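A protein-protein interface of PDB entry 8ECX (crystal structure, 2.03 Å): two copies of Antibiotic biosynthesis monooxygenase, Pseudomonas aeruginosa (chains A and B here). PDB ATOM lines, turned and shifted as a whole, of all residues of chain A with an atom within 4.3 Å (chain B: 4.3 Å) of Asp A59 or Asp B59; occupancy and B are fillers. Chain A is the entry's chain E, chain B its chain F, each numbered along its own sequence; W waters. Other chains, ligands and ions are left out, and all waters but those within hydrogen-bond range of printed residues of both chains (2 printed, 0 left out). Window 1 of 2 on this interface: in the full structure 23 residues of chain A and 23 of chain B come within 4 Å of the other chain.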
ATOM      1  N   VAL A   9      22.814  -9.572  17.915  1.00  0.00           N
ATOM      2  CA  VAL A   9      22.274 -10.182  16.703  1.00  0.00           C
ATOM      3  C   VAL A   9      21.117 -11.084  17.106  1.00  0.00           C
ATOM      4  O   VAL A   9      21.301 -12.011  17.904  1.00  0.00           O
ATOM      5  CB  VAL A   9      23.340 -10.986  15.938  1.00  0.00           C
ATOM      6  CG1 VAL A   9      22.731 -11.659  14.708  1.00  0.00           C
ATOM      7  CG2 VAL A   9      24.513 -10.093  15.547  1.00  0.00           C
ATOM      8  N   LEU A  10      19.933 -10.819  16.558  1.00  0.00           N
ATOM      9  CA  LEU A  10      18.734 -11.601  16.843  1.00  0.00           C
ATOM     10  C   LEU A  10      18.332 -12.365  15.588  1.00  0.00           C
ATOM     11  O   LEU A  10      18.134 -11.765  14.525  1.00  0.00           O
ATOM     12  CB  LEU A  10      17.591 -10.709  17.324  1.00  0.00           C
ATOM     13  CG  LEU A  10      17.297 -10.789  18.823  1.00  0.00           C
ATOM     14  CD1 LEU A  10      16.660 -12.125  19.172  1.00  0.00           C
ATOM     15  CD2 LEU A  10      18.563 -10.560  19.634  1.00  0.00           C
ATOM     16  N   ARG A  43      27.628 -13.695  24.583  1.00  0.00           N
ATOM     17  CA  ARG A  43      26.376 -14.283  25.036  1.00  0.00           C
ATOM     18  C   ARG A  43      25.715 -14.976  23.856  1.00  0.00           C
ATOM     19  O   ARG A  43      25.811 -14.507  22.719  1.00  0.00           O
ATOM     20  CB  ARG A  43      25.444 -13.219  25.633  1.00  0.00           C
ATOM     21  CG  ARG A  43      24.267 -13.779  26.417  1.00  0.00           C
ATOM     22  CD  ARG A  43      23.472 -12.667  27.085  1.00  0.00           C
ATOM     23  NE  ARG A  43      22.658 -11.932  26.124  1.00  0.00           N
ATOM     24  CZ  ARG A  43      22.309 -10.659  26.250  1.00  0.00           C
ATOM     25  NH1 ARG A  43      22.680  -9.940  27.297  1.00  0.00           N
ATOM     26  NH2 ARG A  43      21.566 -10.093  25.303  1.00  0.00           N
ATOM     27  N   PHE A  44      25.041 -16.096  24.133  1.00  0.00           N
ATOM     28  CA  PHE A  44      24.418 -16.884  23.069  1.00  0.00           C
ATOM     29  C   PHE A  44      23.302 -17.715  23.705  1.00  0.00           C
ATOM     30  O   PHE A  44      23.582 -18.705  24.386  1.00  0.00           O
ATOM     31  CB  PHE A  44      25.442 -17.766  22.374  1.00  0.00           C
ATOM     32  CG  PHE A  44      25.081 -18.124  20.961  1.00  0.00           C
ATOM     33  CD1 PHE A  44      23.919 -18.823  20.682  1.00  0.00           C
ATOM     34  CD2 PHE A  44      25.915 -17.770  19.912  1.00  0.00           C
ATOM     35  CE1 PHE A  44      23.588 -19.158  19.384  1.00  0.00           C
ATOM     36  CE2 PHE A  44      25.592 -18.100  18.609  1.00  0.00           C
ATOM     37  CZ  PHE A  44      24.426 -18.795  18.343  1.00  0.00           C
ATOM     38  N   GLU A  45      22.056 -17.318  23.464  1.00  0.00           N
ATOM     39  CA  GLU A  45      20.900 -17.977  24.053  1.00  0.00           C
ATOM     40  C   GLU A  45      19.982 -18.512  22.965  1.00  0.00           C
ATOM     41  O   GLU A  45      19.815 -17.887  21.913  1.00  0.00           O
ATOM     42  CB  GLU A  45      20.120 -17.023  24.965  1.00  0.00           C
ATOM     43  CG  GLU A  45      20.947 -16.453  26.103  1.00  0.00           C
ATOM     44  CD  GLU A  45      20.258 -15.308  26.817  1.00  0.00           C
ATOM     45  OE1 GLU A  45      19.483 -14.576  26.165  1.00  0.00           O
ATOM     46  OE2 GLU A  45      20.489 -15.142  28.033  1.00  0.00           O
ATOM     47  N   ILE A  47      16.074 -19.501  22.281  1.00  0.00           N
ATOM     48  CA  ILE A  47      14.764 -19.143  22.806  1.00  0.00           C
ATOM     49  C   ILE A  47      13.694 -19.791  21.940  1.00  0.00           C
ATOM     50  O   ILE A  47      13.776 -19.760  20.707  1.00  0.00           O
ATOM     51  CB  ILE A  47      14.576 -17.611  22.851  1.00  0.00           C
ATOM     52  CG1 ILE A  47      15.681 -16.961  23.687  1.00  0.00           C
ATOM     53  CG2 ILE A  47      13.212 -17.247  23.414  1.00  0.00           C
ATOM     54  CD1 ILE A  47      15.775 -15.468  23.505  1.00  0.00           C
ATOM     55  N   TYR A  57      14.382 -18.688  18.292  1.00  0.00           N
ATOM     56  CA  TYR A  57      15.186 -17.484  18.154  1.00  0.00           C
ATOM     57  C   TYR A  57      16.566 -17.699  18.759  1.00  0.00           C
ATOM     58  O   TYR A  57      16.729 -18.436  19.735  1.00  0.00           O
ATOM     59  CB  TYR A  57      14.518 -16.271  18.818  1.00  0.00           C
ATOM     60  CG  TYR A  57      13.046 -16.147  18.520  1.00  0.00           C
ATOM     61  CD1 TYR A  57      12.603 -15.526  17.361  1.00  0.00           C
ATOM     62  CD2 TYR A  57      12.097 -16.654  19.396  1.00  0.00           C
ATOM     63  CE1 TYR A  57      11.255 -15.410  17.081  1.00  0.00           C
ATOM     64  CE2 TYR A  57      10.748 -16.542  19.128  1.00  0.00           C
ATOM     65  CZ  TYR A  57      10.333 -15.923  17.967  1.00  0.00           C
ATOM     66  OH  TYR A  57       8.987 -15.811  17.699  1.00  0.00           O
ATOM     67  N   LEU A  58      17.560 -17.049  18.161  1.00  0.00           N
ATOM     68  CA  LEU A  58      18.914 -17.002  18.700  1.00  0.00           C
ATOM     69  C   LEU A  58      19.236 -15.564  19.074  1.00  0.00           C
ATOM     70  O   LEU A  58      19.135 -14.662  18.236  1.00  0.00           O
ATOM     71  CB  LEU A  58      19.939 -17.542  17.701  1.00  0.00           C
ATOM     72  CG  LEU A  58      19.711 -18.939  17.124  1.00  0.00           C
ATOM     73  CD1 LEU A  58      20.833 -19.304  16.169  1.00  0.00           C
ATOM     74  CD2 LEU A  58      19.597 -19.964  18.242  1.00  0.00           C
ATOM     75  N   ASP A  59      19.608 -15.355  20.333  1.00  0.00           N
ATOM     76  CA  ASP A  59      19.971 -14.043  20.851  1.00  0.00           C
ATOM     77  C   ASP A  59      21.475 -14.064  21.100  1.00  0.00           C
ATOM     78  O   ASP A  59      21.942 -14.680  22.065  1.00  0.00           O
ATOM     79  CB  ASP A  59      19.186 -13.735  22.124  1.00  0.00           C
ATOM     80  CG  ASP A  59      19.307 -12.290  22.556  1.00  0.00           C
ATOM     81  OD1 ASP A  59      20.282 -11.616  22.164  1.00  0.00           O
ATOM     82  OD2 ASP A  59      18.416 -11.831  23.297  1.00  0.00           O
ATOM     83  N   GLU A  60      22.225 -13.396  20.230  1.00  0.00           N
ATOM     84  CA  GLU A  60      23.680 -13.451  20.227  1.00  0.00           C
ATOM     85  C   GLU A  60      24.257 -12.077  20.529  1.00  0.00           C
ATOM     86  O   GLU A  60      23.734 -11.060  20.064  1.00  0.00           O
ATOM     87  CB  GLU A  60      24.194 -13.944  18.876  1.00  0.00           C
ATOM     88  CG  GLU A  60      23.456 -15.163  18.361  1.00  0.00           C
ATOM     89  CD  GLU A  60      23.793 -15.491  16.922  1.00  0.00           C
ATOM     90  OE1 GLU A  60      24.746 -14.895  16.379  1.00  0.00           O
ATOM     91  OE2 GLU A  60      23.094 -16.338  16.327  1.00  0.00           O
ATOM     92  N   VAL B   9      11.449 -11.123  26.306  1.00  0.00           N
ATOM     93  CA  VAL B   9      10.537 -10.227  25.604  1.00  0.00           C
ATOM     94  C   VAL B   9      11.374  -9.284  24.753  1.00  0.00           C
ATOM     95  O   VAL B   9      12.256  -8.592  25.275  1.00  0.00           O
ATOM     96  CB  VAL B   9       9.652  -9.430  26.577  1.00  0.00           C
ATOM     97  CG1 VAL B   9       8.713  -8.514  25.810  1.00  0.00           C
ATOM     98  CG2 VAL B   9       8.867 -10.372  27.482  1.00  0.00           C
ATOM     99  N   LEU B  10      11.100  -9.252  23.451  1.00  0.00           N
ATOM    100  CA  LEU B  10      11.830  -8.403  22.515  1.00  0.00           C
ATOM    101  C   LEU B  10      10.862  -7.400  21.906  1.00  0.00           C
ATOM    102  O   LEU B  10       9.872  -7.790  21.279  1.00  0.00           O
ATOM    103  CB  LEU B  10      12.507  -9.232  21.423  1.00  0.00           C
ATOM    104  CG  LEU B  10      13.536  -8.471  20.583  1.00  0.00           C
ATOM    105  CD1 LEU B  10      14.723  -8.046  21.446  1.00  0.00           C
ATOM    106  CD2 LEU B  10      13.996  -9.321  19.417  1.00  0.00           C
ATOM    107  N   ARG B  43      16.906  -8.805  33.178  1.00  0.00           N
ATOM    108  CA  ARG B  43      17.735  -8.161  32.171  1.00  0.00           C
ATOM    109  C   ARG B  43      16.869  -7.213  31.355  1.00  0.00           C
ATOM    110  O   ARG B  43      15.705  -7.509  31.075  1.00  0.00           O
ATOM    111  CB  ARG B  43      18.414  -9.197  31.265  1.00  0.00           C
ATOM    112  CG  ARG B  43      19.561  -8.659  30.418  1.00  0.00           C
ATOM    113  CD  ARG B  43      20.330  -9.805  29.772  1.00  0.00           C
ATOM    114  NE  ARG B  43      19.639 -10.331  28.600  1.00  0.00           N
ATOM    115  CZ  ARG B  43      19.732 -11.583  28.172  1.00  0.00           C
ATOM    116  NH1 ARG B  43      20.454 -12.483  28.819  1.00  0.00           N
ATOM    117  NH2 ARG B  43      19.077 -11.942  27.072  1.00  0.00           N
ATOM    118  N   PHE B  44      17.447  -6.068  30.987  1.00  0.00           N
ATOM    119  CA  PHE B  44      16.711  -5.043  30.250  1.00  0.00           C
ATOM    120  C   PHE B  44      17.744  -4.226  29.475  1.00  0.00           C
ATOM    121  O   PHE B  44      18.460  -3.414  30.067  1.00  0.00           O
ATOM    122  CB  PHE B  44      15.900  -4.168  31.190  1.00  0.00           C
ATOM    123  CG  PHE B  44      14.689  -3.554  30.556  1.00  0.00           C
ATOM    124  CD1 PHE B  44      14.817  -2.630  29.530  1.00  0.00           C
ATOM    125  CD2 PHE B  44      13.420  -3.894  30.990  1.00  0.00           C
ATOM    126  CE1 PHE B  44      13.701  -2.059  28.949  1.00  0.00           C
ATOM    127  CE2 PHE B  44      12.302  -3.327  30.413  1.00  0.00           C
ATOM    128  CZ  PHE B  44      12.443  -2.409  29.390  1.00  0.00           C
ATOM    129  N   GLU B  45      17.810  -4.447  28.165  1.00  0.00           N
ATOM    130  CA  GLU B  45      18.813  -3.821  27.317  1.00  0.00           C
ATOM    131  C   GLU B  45      18.142  -2.933  26.279  1.00  0.00           C
ATOM    132  O   GLU B  45      17.104  -3.294  25.714  1.00  0.00           O
ATOM    133  CB  GLU B  45      19.681  -4.880  26.625  1.00  0.00           C
ATOM    134  CG  GLU B  45      20.460  -5.761  27.588  1.00  0.00           C
ATOM    135  CD  GLU B  45      21.252  -6.844  26.882  1.00  0.00           C
ATOM    136  OE1 GLU B  45      20.747  -7.395  25.881  1.00  0.00           O
ATOM    137  OE2 GLU B  45      22.378  -7.149  27.331  1.00  0.00           O
ATOM    138  N   ILE B  47      18.808  -1.297  22.631  1.00  0.00           N
ATOM    139  CA  ILE B  47      19.642  -1.607  21.476  1.00  0.00           C
ATOM    140  C   ILE B  47      19.224  -0.725  20.308  1.00  0.00           C
ATOM    141  O   ILE B  47      18.035  -0.635  19.986  1.00  0.00           O
ATOM    142  CB  ILE B  47      19.549  -3.096  21.089  1.00  0.00           C
ATOM    143  CG1 ILE B  47      19.971  -3.983  22.264  1.00  0.00           C
ATOM    144  CG2 ILE B  47      20.402  -3.386  19.864  1.00  0.00           C
ATOM    145  CD1 ILE B  47      19.614  -5.437  22.083  1.00  0.00           C
ATOM    146  N   TYR B  57      15.467  -1.303  19.861  1.00  0.00           N
ATOM    147  CA  TYR B  57      14.942  -2.561  20.368  1.00  0.00           C
ATOM    148  C   TYR B  57      15.170  -2.651  21.870  1.00  0.00           C
ATOM    149  O   TYR B  57      16.208  -2.217  22.378  1.00  0.00           O
ATOM    150  CB  TYR B  57      15.588  -3.763  19.671  1.00  0.00           C
ATOM    151  CG  TYR B  57      15.695  -3.604  18.175  1.00  0.00           C
ATOM    152  CD1 TYR B  57      14.623  -3.909  17.347  1.00  0.00           C
ATOM    153  CD2 TYR B  57      16.865  -3.141  17.591  1.00  0.00           C
ATOM    154  CE1 TYR B  57      14.714  -3.763  15.977  1.00  0.00           C
ATOM    155  CE2 TYR B  57      16.966  -2.987  16.224  1.00  0.00           C
ATOM    156  CZ  TYR B  57      15.889  -3.301  15.422  1.00  0.00           C
ATOM    157  OH  TYR B  57      15.989  -3.153  14.057  1.00  0.00           O
ATOM    158  N   LEU B  58      14.190  -3.210  22.574  1.00  0.00           N
ATOM    159  CA  LEU B  58      14.305  -3.506  23.996  1.00  0.00           C
ATOM    160  C   LEU B  58      14.394  -5.015  24.165  1.00  0.00           C
ATOM    161  O   LEU B  58      13.480  -5.744  23.762  1.00  0.00           O
ATOM    162  CB  LEU B  58      13.118  -2.953  24.784  1.00  0.00           C
ATOM    163  CG  LEU B  58      12.826  -1.455  24.698  1.00  0.00           C
ATOM    164  CD1 LEU B  58      11.731  -1.075  25.681  1.00  0.00           C
ATOM    165  CD2 LEU B  58      14.086  -0.634  24.937  1.00  0.00           C
ATOM    166  N   ASP B  59      15.489  -5.479  24.752  1.00  0.00           N
ATOM    167  CA  ASP B  59      15.720  -6.898  24.994  1.00  0.00           C
ATOM    168  C   ASP B  59      15.561  -7.133  26.491  1.00  0.00           C
ATOM    169  O   ASP B  59      16.434  -6.755  27.280  1.00  0.00           O
ATOM    170  CB  ASP B  59      17.106  -7.309  24.501  1.00  0.00           C
ATOM    171  CG  ASP B  59      17.279  -8.811  24.421  1.00  0.00           C
ATOM    172  OD1 ASP B  59      16.403  -9.553  24.912  1.00  0.00           O
ATOM    173  OD2 ASP B  59      18.297  -9.247  23.849  1.00  0.00           O
ATOM    174  N   GLU B  60      14.448  -7.752  26.879  1.00  0.00           N
ATOM    175  CA  GLU B  60      14.058  -7.880  28.276  1.00  0.00           C
ATOM    176  C   GLU B  60      13.990  -9.349  28.668  1.00  0.00           C
ATOM    177  O   GLU B  60      13.558 -10.192  27.877  1.00  0.00           O
ATOM    178  CB  GLU B  60      12.698  -7.218  28.526  1.00  0.00           C
ATOM    179  CG  GLU B  60      12.519  -5.888  27.811  1.00  0.00           C
ATOM    180  CD  GLU B  60      11.099  -5.374  27.891  1.00  0.00           C
ATOM    181  OE1 GLU B  60      10.292  -5.985  28.621  1.00  0.00           O
ATOM    182  OE2 GLU B  60      10.787  -4.366  27.222  1.00  0.00           O
HETATM  183  O   HOH W   1      20.425  -8.890  22.395  1.00  0.00           O
HETATM  184  O   HOH W   2      16.363 -12.511  24.607  1.00  0.00           O
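The side-chain carboxylate of Glu B45 is in salt-bridge range of the guanidinium group of Arg A43, 2.8 Å away.
The guanidinium group (NH2) of Arg A43 lies within salt-bridge range of the side-chain carboxylate (OD2) of Asp B59, 3.7 Å away.
The guanidinium group of Arg B43 is in salt-bridge range of the side-chain carboxylate of Glu A45 (2.8 Å).
The side-chain carboxylate of Asp A59 lies within salt-bridge range of the guanidinium group of Arg B43 (3.8 Å).
OD2 of Asp A59 sits close to OD2 of Asp B59, 2.6 Å away.
NE of Arg B43 sits close to NH1 of Arg A43 (3.3 Å).
The guanidinium group of Arg A43 is in salt-bridge range of the side-chain carboxylate of Asp A59, at 3.7 Å.
The backbone carbonyl oxygen (O) of Asp A59 sits at hydrogen-bond distance from the backbone NH (N) of Glu A45.
The backbone carbonyl oxygen (O) of Asp B59 sits at hydrogen-bond distance from the backbone NH (N) of Glu B45.
CD2 of Leu B10 touches CG of Leu A10, at 3.7 Å.
Of the printed residues of chain B, Asp A59 touches Arg B43 (3.8 Å) and Asp B59 (2.6 Å).
Asp B59 touches just these residues of chain A: Arg A43 and Asp A59.
Of the printed residues of chain A, Arg B43 touches Arg A43, Glu A45 and Asp A59.
Printed residues of chain A within 4 Å of Leu B10: Leu A10 (3.7 Å).
Phe B44 touches none of the printed residues of chain A.
Ile A47 touches none of the printed residues of chain B.
The nearest printed residue of chain B that does not touch Asp A59 is Leu B10 (5.6 Å).
The nearest printed residue of chain A that does not touch Asp B59 is Leu A10 (4.4 Å).
Of the 10 printed residues of chain B, 4 touch a printed residue of chain A.
Printed residues of chain B that touch a printed residue of chain A: Leu B10, Arg B43, Glu B45 and Asp B59.
Leu B10 touches its own counterpart, Leu A10.
Arg A43 touches its own counterpart, Arg B43.
Arg A43 touches Glu B45, and with the chains exchanged Glu A45 touches Arg B43.
Asp A59 touches its own counterpart, Asp B59.
Positions printed for both chains: 9, 10, 43, 44, 45, 47, 57, 58, 59 and 60.
Of the 7 pairs that touch across the chains among the printed residues, 7 have their exchanged pair printed and touching as well.
Water W2 lies within hydrogen-bond range of the side-chain carboxylate of Asp A59 (2.5 Å) and the side-chain carboxylate of Asp B59 (3.0 Å).
Water W1 lies within hydrogen-bond range of the side-chain carboxylate (OD2) of Asp B59 (2.6 Å), the side-chain carboxylate (OD1) of Asp A59 (2.7 Å) and the guanidinium group (NH2) of Arg A43 (3.3 Å).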
